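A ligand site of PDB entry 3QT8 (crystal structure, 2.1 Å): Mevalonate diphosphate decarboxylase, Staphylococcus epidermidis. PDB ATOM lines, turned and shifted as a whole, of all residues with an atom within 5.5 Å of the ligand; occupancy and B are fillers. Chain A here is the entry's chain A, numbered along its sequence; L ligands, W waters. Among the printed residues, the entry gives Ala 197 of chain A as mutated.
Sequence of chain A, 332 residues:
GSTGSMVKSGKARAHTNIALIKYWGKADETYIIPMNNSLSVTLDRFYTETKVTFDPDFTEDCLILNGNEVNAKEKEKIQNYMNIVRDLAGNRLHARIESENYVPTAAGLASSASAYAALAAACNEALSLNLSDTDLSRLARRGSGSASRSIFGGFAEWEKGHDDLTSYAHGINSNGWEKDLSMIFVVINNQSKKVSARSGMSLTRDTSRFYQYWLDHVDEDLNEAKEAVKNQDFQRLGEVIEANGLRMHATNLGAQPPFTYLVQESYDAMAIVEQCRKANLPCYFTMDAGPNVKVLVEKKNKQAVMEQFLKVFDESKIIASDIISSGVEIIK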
ATOM      1  N   ASN A  17     -18.729  21.996  13.119  1.00  0.00           N
ATOM      2  CA  ASN A  17     -19.124  20.594  13.238  1.00  0.00           C
ATOM      3  C   ASN A  17     -20.299  20.278  12.327  1.00  0.00           C
ATOM      4  O   ASN A  17     -21.144  21.148  12.061  1.00  0.00           O
ATOM      5  CB  ASN A  17     -19.486  20.251  14.682  1.00  0.00           C
ATOM      6  CG  ASN A  17     -20.785  20.862  15.122  1.00  0.00           C
ATOM      7  OD1 ASN A  17     -21.858  20.311  14.874  1.00  0.00           O
ATOM      8  ND2 ASN A  17     -20.704  22.008  15.776  1.00  0.00           N
ATOM      9  N   ALA A  19     -23.642  17.772  11.946  1.00  0.00           N
ATOM     10  CA  ALA A  19     -24.562  16.866  12.615  1.00  0.00           C
ATOM     11  C   ALA A  19     -24.706  15.566  11.828  1.00  0.00           C
ATOM     12  O   ALA A  19     -24.995  15.608  10.623  1.00  0.00           O
ATOM     13  CB  ALA A  19     -25.915  17.516  12.827  1.00  0.00           C
ATOM     14  N   ILE A  21     -26.574  13.013  13.629  1.00  0.00           N
ATOM     15  CA  ILE A  21     -27.973  12.985  14.027  1.00  0.00           C
ATOM     16  C   ILE A  21     -28.409  14.442  14.195  1.00  0.00           C
ATOM     17  O   ILE A  21     -27.840  15.159  14.992  1.00  0.00           O
ATOM     18  CB  ILE A  21     -28.199  12.207  15.320  1.00  0.00           C
ATOM     19  CG1 ILE A  21     -27.763  10.766  15.125  1.00  0.00           C
ATOM     20  CG2 ILE A  21     -29.667  12.274  15.702  1.00  0.00           C
ATOM     21  CD1 ILE A  21     -28.718   9.970  14.244  1.00  0.00           C
ATOM     22  N   LYS A  22     -29.432  14.845  13.437  1.00  0.00           N
ATOM     23  CA  LYS A  22     -29.803  16.254  13.270  1.00  0.00           C
ATOM     24  C   LYS A  22     -30.565  16.912  14.411  1.00  0.00           C
ATOM     25  O   LYS A  22     -31.513  16.356  14.964  1.00  0.00           O
ATOM     26  CB  LYS A  22     -30.636  16.442  11.983  1.00  0.00           C
ATOM     27  CG  LYS A  22     -30.001  15.907  10.707  1.00  0.00           C
ATOM     28  CD  LYS A  22     -28.648  16.521  10.415  1.00  0.00           C
ATOM     29  CE  LYS A  22     -28.270  16.302   8.979  1.00  0.00           C
ATOM     30  NZ  LYS A  22     -26.863  16.693   8.675  1.00  0.00           N
ATOM     31  N   TYR A  23     -30.153  18.135  14.729  1.00  0.00           N
ATOM     32  CA  TYR A  23     -30.952  19.056  15.520  1.00  0.00           C
ATOM     33  C   TYR A  23     -31.882  19.752  14.538  1.00  0.00           C
ATOM     34  O   TYR A  23     -31.440  20.266  13.526  1.00  0.00           O
ATOM     35  CB  TYR A  23     -30.023  20.049  16.204  1.00  0.00           C
ATOM     36  CG  TYR A  23     -30.559  21.435  16.451  1.00  0.00           C
ATOM     37  CD1 TYR A  23     -31.764  21.648  17.100  1.00  0.00           C
ATOM     38  CD2 TYR A  23     -29.804  22.546  16.099  1.00  0.00           C
ATOM     39  CE1 TYR A  23     -32.225  22.951  17.349  1.00  0.00           C
ATOM     40  CE2 TYR A  23     -30.250  23.826  16.334  1.00  0.00           C
ATOM     41  CZ  TYR A  23     -31.445  24.020  16.958  1.00  0.00           C
ATOM     42  OH  TYR A  23     -31.858  25.326  17.187  1.00  0.00           O
ATOM     43  N   TRP A  24     -33.172  19.748  14.809  1.00  0.00           N
ATOM     44  CA  TRP A  24     -34.111  20.298  13.839  1.00  0.00           C
ATOM     45  C   TRP A  24     -35.402  20.612  14.537  1.00  0.00           C
ATOM     46  O   TRP A  24     -36.197  19.708  14.827  1.00  0.00           O
ATOM     47  CB  TRP A  24     -34.315  19.316  12.671  1.00  0.00           C
ATOM     48  CG  TRP A  24     -34.949  19.976  11.488  1.00  0.00           C
ATOM     49  CD1 TRP A  24     -36.171  19.681  10.937  1.00  0.00           C
ATOM     50  CD2 TRP A  24     -34.407  21.049  10.734  1.00  0.00           C
ATOM     51  NE1 TRP A  24     -36.415  20.514   9.862  1.00  0.00           N
ATOM     52  CE2 TRP A  24     -35.344  21.374   9.718  1.00  0.00           C
ATOM     53  CE3 TRP A  24     -33.216  21.781  10.797  1.00  0.00           C
ATOM     54  CZ2 TRP A  24     -35.128  22.394   8.789  1.00  0.00           C
ATOM     55  CZ3 TRP A  24     -33.002  22.799   9.892  1.00  0.00           C
ATOM     56  CH2 TRP A  24     -33.950  23.096   8.890  1.00  0.00           C
ATOM     57  N   LYS A  26     -36.933  23.688  17.573  1.00  0.00           N
ATOM     58  CA  LYS A  26     -36.676  24.083  18.957  1.00  0.00           C
ATOM     59  C   LYS A  26     -37.884  23.901  19.834  1.00  0.00           C
ATOM     60  O   LYS A  26     -39.017  24.217  19.433  1.00  0.00           O
ATOM     61  CB  LYS A  26     -36.257  25.565  19.032  1.00  0.00           C
ATOM     62  CG  LYS A  26     -34.962  25.926  18.316  1.00  0.00           C
ATOM     63  CD  LYS A  26     -34.894  27.439  18.154  1.00  0.00           C
ATOM     64  CE  LYS A  26     -33.594  27.927  17.502  1.00  0.00           C
ATOM     65  NZ  LYS A  26     -33.435  27.431  16.110  1.00  0.00           N
ATOM     66  N   ILE A  32     -32.967  28.825  22.916  1.00  0.00           N
ATOM     67  CA  ILE A  32     -32.471  27.766  22.036  1.00  0.00           C
ATOM     68  C   ILE A  32     -32.333  26.415  22.723  1.00  0.00           C
ATOM     69  O   ILE A  32     -31.247  25.900  22.949  1.00  0.00           O
ATOM     70  CB  ILE A  32     -31.234  28.189  21.282  1.00  0.00           C
ATOM     71  CG1 ILE A  32     -31.510  29.542  20.639  1.00  0.00           C
ATOM     72  CG2 ILE A  32     -30.869  27.129  20.220  1.00  0.00           C
ATOM     73  CD1 ILE A  32     -30.410  30.083  19.770  1.00  0.00           C
ATOM     74  N   SER A  38     -28.738  15.796  19.598  1.00  0.00           N
ATOM     75  CA  SER A  38     -28.084  15.656  18.325  1.00  0.00           C
ATOM     76  C   SER A  38     -26.703  15.098  18.531  1.00  0.00           C
ATOM     77  O   SER A  38     -26.184  15.131  19.640  1.00  0.00           O
ATOM     78  CB  SER A  38     -28.056  16.992  17.554  1.00  0.00           C
ATOM     79  OG  SER A  38     -27.517  18.031  18.331  1.00  0.00           O
ATOM     80  N   SER A 112     -22.020  29.316  11.568  1.00  0.00           N
ATOM     81  CA  SER A 112     -22.673  29.657  12.815  1.00  0.00           C
ATOM     82  C   SER A 112     -22.138  28.880  14.041  1.00  0.00           C
ATOM     83  O   SER A 112     -22.065  29.417  15.138  1.00  0.00           O
ATOM     84  CB  SER A 112     -24.176  29.474  12.677  1.00  0.00           C
ATOM     85  OG  SER A 112     -24.828  29.961  13.827  1.00  0.00           O
ATOM     86  N   GLY A 143     -26.313  31.486  21.369  1.00  0.00           N
ATOM     87  CA  GLY A 143     -26.064  32.190  20.118  1.00  0.00           C
ATOM     88  C   GLY A 143     -26.559  31.393  18.912  1.00  0.00           C
ATOM     89  O   GLY A 143     -27.227  31.934  18.021  1.00  0.00           O
ATOM     90  N   SER A 144     -26.214  30.102  18.883  1.00  0.00           N
ATOM     91  CA  SER A 144     -26.708  29.179  17.857  1.00  0.00           C
ATOM     92  C   SER A 144     -26.615  27.758  18.378  1.00  0.00           C
ATOM     93  O   SER A 144     -25.579  27.374  18.930  1.00  0.00           O
ATOM     94  CB  SER A 144     -25.863  29.328  16.579  1.00  0.00           C
ATOM     95  OG  SER A 144     -26.195  28.325  15.628  1.00  0.00           O
ATOM     96  N   GLY A 145     -27.676  26.972  18.212  1.00  0.00           N
ATOM     97  CA  GLY A 145     -27.741  25.623  18.773  1.00  0.00           C
ATOM     98  C   GLY A 145     -26.562  24.729  18.436  1.00  0.00           C
ATOM     99  O   GLY A 145     -25.913  24.176  19.324  1.00  0.00           O
ATOM    100  N   SER A 146     -26.294  24.564  17.149  1.00  0.00           N
ATOM    101  CA  SER A 146     -25.126  23.819  16.674  1.00  0.00           C
ATOM    102  C   SER A 146     -23.792  24.303  17.284  1.00  0.00           C
ATOM    103  O   SER A 146     -22.813  23.561  17.288  1.00  0.00           O
ATOM    104  CB  SER A 146     -25.038  23.901  15.159  1.00  0.00           C
ATOM    105  OG  SER A 146     -25.003  25.253  14.722  1.00  0.00           O
ATOM    106  N   ALA A 147     -23.738  25.531  17.781  1.00  0.00           N
ATOM    107  CA  ALA A 147     -22.493  26.033  18.347  1.00  0.00           C
ATOM    108  C   ALA A 147     -22.137  25.315  19.634  1.00  0.00           C
ATOM    109  O   ALA A 147     -20.956  25.248  20.026  1.00  0.00           O
ATOM    110  CB  ALA A 147     -22.573  27.544  18.582  1.00  0.00           C
ATOM    111  N   ARG A 149     -21.938  22.349  20.250  1.00  0.00           N
ATOM    112  CA  ARG A 149     -21.136  21.154  20.026  1.00  0.00           C
ATOM    113  C   ARG A 149     -19.711  21.449  19.585  1.00  0.00           C
ATOM    114  O   ARG A 149     -18.818  20.613  19.775  1.00  0.00           O
ATOM    115  CB  ARG A 149     -21.822  20.226  19.017  1.00  0.00           C
ATOM    116  CG  ARG A 149     -23.320  20.024  19.252  1.00  0.00           C
ATOM    117  CD  ARG A 149     -23.941  19.047  18.242  1.00  0.00           C
ATOM    118  NE  ARG A 149     -23.777  19.522  16.871  1.00  0.00           N
ATOM    119  CZ  ARG A 149     -24.789  19.869  16.084  1.00  0.00           C
ATOM    120  NH1 ARG A 149     -26.040  19.758  16.523  1.00  0.00           N
ATOM    121  NH2 ARG A 149     -24.538  20.321  14.860  1.00  0.00           N
ATOM    122  N   ALA A 197     -31.619  28.183   8.395  1.00  0.00           N
ATOM    123  CA  ALA A 197     -31.839  27.019   9.248  1.00  0.00           C
ATOM    124  C   ALA A 197     -32.835  27.308  10.367  1.00  0.00           C
ATOM    125  O   ALA A 197     -33.768  26.553  10.606  1.00  0.00           O
ATOM    126  CB  ALA A 197     -30.522  26.482   9.860  1.00  0.00           C
ATOM    127  N   ARG A 198     -32.608  28.412  11.082  1.00  0.00           N
ATOM    128  CA  ARG A 198     -33.459  28.808  12.206  1.00  0.00           C
ATOM    129  C   ARG A 198     -34.896  28.946  11.738  1.00  0.00           C
ATOM    130  O   ARG A 198     -35.816  28.393  12.343  1.00  0.00           O
ATOM    131  CB  ARG A 198     -32.964  30.138  12.787  1.00  0.00           C
ATOM    132  CG  ARG A 198     -33.833  30.751  13.906  1.00  0.00           C
ATOM    133  CD  ARG A 198     -33.030  31.833  14.708  1.00  0.00           C
ATOM    134  NE  ARG A 198     -31.748  31.300  15.177  1.00  0.00           N
ATOM    135  CZ  ARG A 198     -30.828  31.986  15.877  1.00  0.00           C
ATOM    136  NH1 ARG A 198     -31.065  33.240  16.222  1.00  0.00           N
ATOM    137  NH2 ARG A 198     -29.678  31.403  16.231  1.00  0.00           N
ATOM    138  N   MET A 201     -36.330  25.423  10.282  1.00  0.00           N
ATOM    139  CA  MET A 201     -36.656  24.432  11.314  1.00  0.00           C
ATOM    140  C   MET A 201     -37.888  24.877  12.085  1.00  0.00           C
ATOM    141  O   MET A 201     -38.684  24.057  12.510  1.00  0.00           O
ATOM    142  CB  MET A 201     -35.449  24.167  12.237  1.00  0.00           C
ATOM    143  CG  MET A 201     -35.223  25.197  13.345  1.00  0.00           C
ATOM    144  SD  MET A 201     -33.935  24.664  14.510  1.00  0.00           S
ATOM    145  CE  MET A 201     -32.525  24.579  13.426  1.00  0.00           C
ATOM    146  N   MET A 248     -34.981  14.005   8.331  1.00  0.00           N
ATOM    147  CA  MET A 248     -35.038  15.441   8.608  1.00  0.00           C
ATOM    148  C   MET A 248     -35.533  16.207   7.402  1.00  0.00           C
ATOM    149  O   MET A 248     -36.385  17.087   7.514  1.00  0.00           O
ATOM    150  CB  MET A 248     -33.666  15.990   9.004  1.00  0.00           C
ATOM    151  CG  MET A 248     -33.728  17.476   9.399  1.00  0.00           C
ATOM    152  SD  MET A 248     -32.200  18.382   9.126  1.00  0.00           S
ATOM    153  CE  MET A 248     -32.501  18.998   7.470  1.00  0.00           C
ATOM    154  N   MET A 287     -27.168  15.947   4.607  1.00  0.00           N
ATOM    155  CA  MET A 287     -27.305  17.314   4.106  1.00  0.00           C
ATOM    156  C   MET A 287     -27.874  18.163   5.231  1.00  0.00           C
ATOM    157  O   MET A 287     -28.653  17.664   6.052  1.00  0.00           O
ATOM    158  CB  MET A 287     -28.254  17.369   2.896  1.00  0.00           C
ATOM    159  CG  MET A 287     -27.721  16.727   1.644  1.00  0.00           C
ATOM    160  SD  MET A 287     -27.796  14.928   1.668  1.00  0.00           S
ATOM    161  CE  MET A 287     -29.524  14.651   1.999  1.00  0.00           C
ATOM    162  N   ASP A 288     -27.498  19.439   5.245  1.00  0.00           N
ATOM    163  CA  ASP A 288     -27.983  20.369   6.253  1.00  0.00           C
ATOM    164  C   ASP A 288     -28.971  21.356   5.628  1.00  0.00           C
ATOM    165  O   ASP A 288     -29.837  20.942   4.859  1.00  0.00           O
ATOM    166  CB  ASP A 288     -26.797  21.024   6.972  1.00  0.00           C
ATOM    167  CG  ASP A 288     -26.025  20.004   7.824  1.00  0.00           C
ATOM    168  OD1 ASP A 288     -26.644  19.374   8.691  1.00  0.00           O
ATOM    169  OD2 ASP A 288     -24.810  19.814   7.597  1.00  0.00           O
ATOM    170  N   ALA A 289     -28.884  22.642   5.945  1.00  0.00           N
ATOM    171  CA  ALA A 289     -29.858  23.606   5.427  1.00  0.00           C
ATOM    172  C   ALA A 289     -29.448  24.157   4.073  1.00  0.00           C
ATOM    173  O   ALA A 289     -29.277  25.355   3.909  1.00  0.00           O
ATOM    174  CB  ALA A 289     -30.082  24.746   6.418  1.00  0.00           C
HETATM  175  O1  LIG L   1     -26.671  21.262  13.020  1.00  0.00           O
HETATM  176  O2  LIG L   1     -28.771  28.783  15.197  1.00  0.00           O
HETATM  177  O3  LIG L   1     -27.609  25.759  14.786  1.00  0.00           O
HETATM  178  O4  LIG L   1     -27.975  19.819  14.051  1.00  0.00           O
HETATM  179  O5  LIG L   1     -27.546  22.255  10.642  1.00  0.00           O
HETATM  180  O6  LIG L   1     -31.250  28.613  15.032  1.00  0.00           O
HETATM  181  O7  LIG L   1     -30.022  27.238  16.687  1.00  0.00           O
HETATM  182  O8  LIG L   1     -27.895  26.994  12.632  1.00  0.00           O
HETATM  183  F1  LIG L   1     -29.742  22.398   8.899  1.00  0.00           F
HETATM  184  C1  LIG L   1     -29.488  21.388   9.756  1.00  0.00           C
HETATM  185  C2  LIG L   1     -28.561  23.789  12.405  1.00  0.00           C
HETATM  186  C3  LIG L   1     -29.436  22.681  11.850  1.00  0.00           C
HETATM  187  C4  LIG L   1     -28.549  20.384  11.801  1.00  0.00           C
HETATM  188  O9  LIG L   1     -29.191  24.766  13.131  1.00  0.00           O
HETATM  189  O10 LIG L   1     -29.868  26.812  14.189  1.00  0.00           O
HETATM  190  C5  LIG L   1     -27.681  20.481  13.023  1.00  0.00           C
HETATM  191  C6  LIG L   1     -28.750  21.670  11.012  1.00  0.00           C
HETATM  192  P1  LIG L   1     -29.960  27.864  15.305  1.00  0.00           P
HETATM  193  P2  LIG L   1     -28.560  26.108  13.664  1.00  0.00           P
HETATM  194  O   HOH W   1     -24.552  20.070  10.562  1.00  0.00           O
HETATM  195  O   HOH W   2     -27.992  29.625  12.905  1.00  0.00           O
HETATM  196  O   HOH W   3     -26.567  24.314   9.306  1.00  0.00           O
HETATM  197  O   HOH W   4     -25.674  26.285  10.759  1.00  0.00           O
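O2 of the ligand sits at hydrogen-bond distance from OG of Ser 144.
N of Ser 146 sits at hydrogen-bond distance from O3 of the ligand (3.0 Å).
The side-chain hydroxyl of Ser 146 sits at hydrogen-bond distance from an oxygen (O3) of the ligand.
An oxygen (O4) of the ligand is in hydrogen-bond range of the backbone NH of Tyr 23, 2.8 Å away.
The side-chain hydroxyl of Tyr 23 sits at hydrogen-bond distance from an oxygen (O7) of the ligand.
The side-chain amino group of Lys 26 is in salt-bridge range of an oxygen (O6) of the ligand (2.7 Å).
O6 of the ligand lies within salt-bridge range of NE of Arg 198 (2.7 Å).
The backbone NH of Gly 145 lies within hydrogen-bond range of an oxygen (O7) of the ligand, at 2.8 Å.
The guanidinium group (NH2) of Arg 149 is in salt-bridge range of an oxygen (O1) of the ligand (3.0 Å).
The side-chain hydroxyl (OG) of Ser 144 sits at hydrogen-bond distance from the side-chain hydroxyl (OG) of Ser 112, 2.8 Å away.
The side-chain amide nitrogen (ND2) of Asn 17 sits at hydrogen-bond distance from the backbone carbonyl oxygen (O) of Ser 146 (3.0 Å).
The side-chain hydroxyl of Tyr 23 sits at hydrogen-bond distance from the side-chain amino group of Lys 26.
OH of Tyr 23 lies within hydrogen-bond range of SD of Met 201, 3.5 Å away.
The guanidinium group of Arg 198 is in hydrogen-bond range of the backbone carbonyl oxygen of Gly 143 (3.1 Å).
The guanidinium group of Arg 149 is in hydrogen-bond range of the side-chain hydroxyl of Ser 38, at 2.9 Å.
The backbone carbonyl oxygen of Ala 19 is in hydrogen-bond range of the side-chain amino group of Lys 22 (2.9 Å).
The side-chain amino group (NZ) of Lys 22 sits close to the backbone carbonyl oxygen (O) of Met 287 (3.3 Å).
A fluorine (F1) of the ligand lies close to the backbone NH (N) of Ala 289, at 3.1 Å.
Merely in contact with the ligand: Ala 19, Lys 22, Trp 24, Ile 32, Ala 197, Met 201 and Asp 288.
Water W2 lies within hydrogen-bond range of O2 of the ligand (2.6 Å) and OG of Ser 112 (3.3 Å).
Water W1 lies within hydrogen-bond range of N of Ala 19 (2.8 Å), OD1 of Asp 288 (2.9 Å) and O1 of the ligand (3.5 Å).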
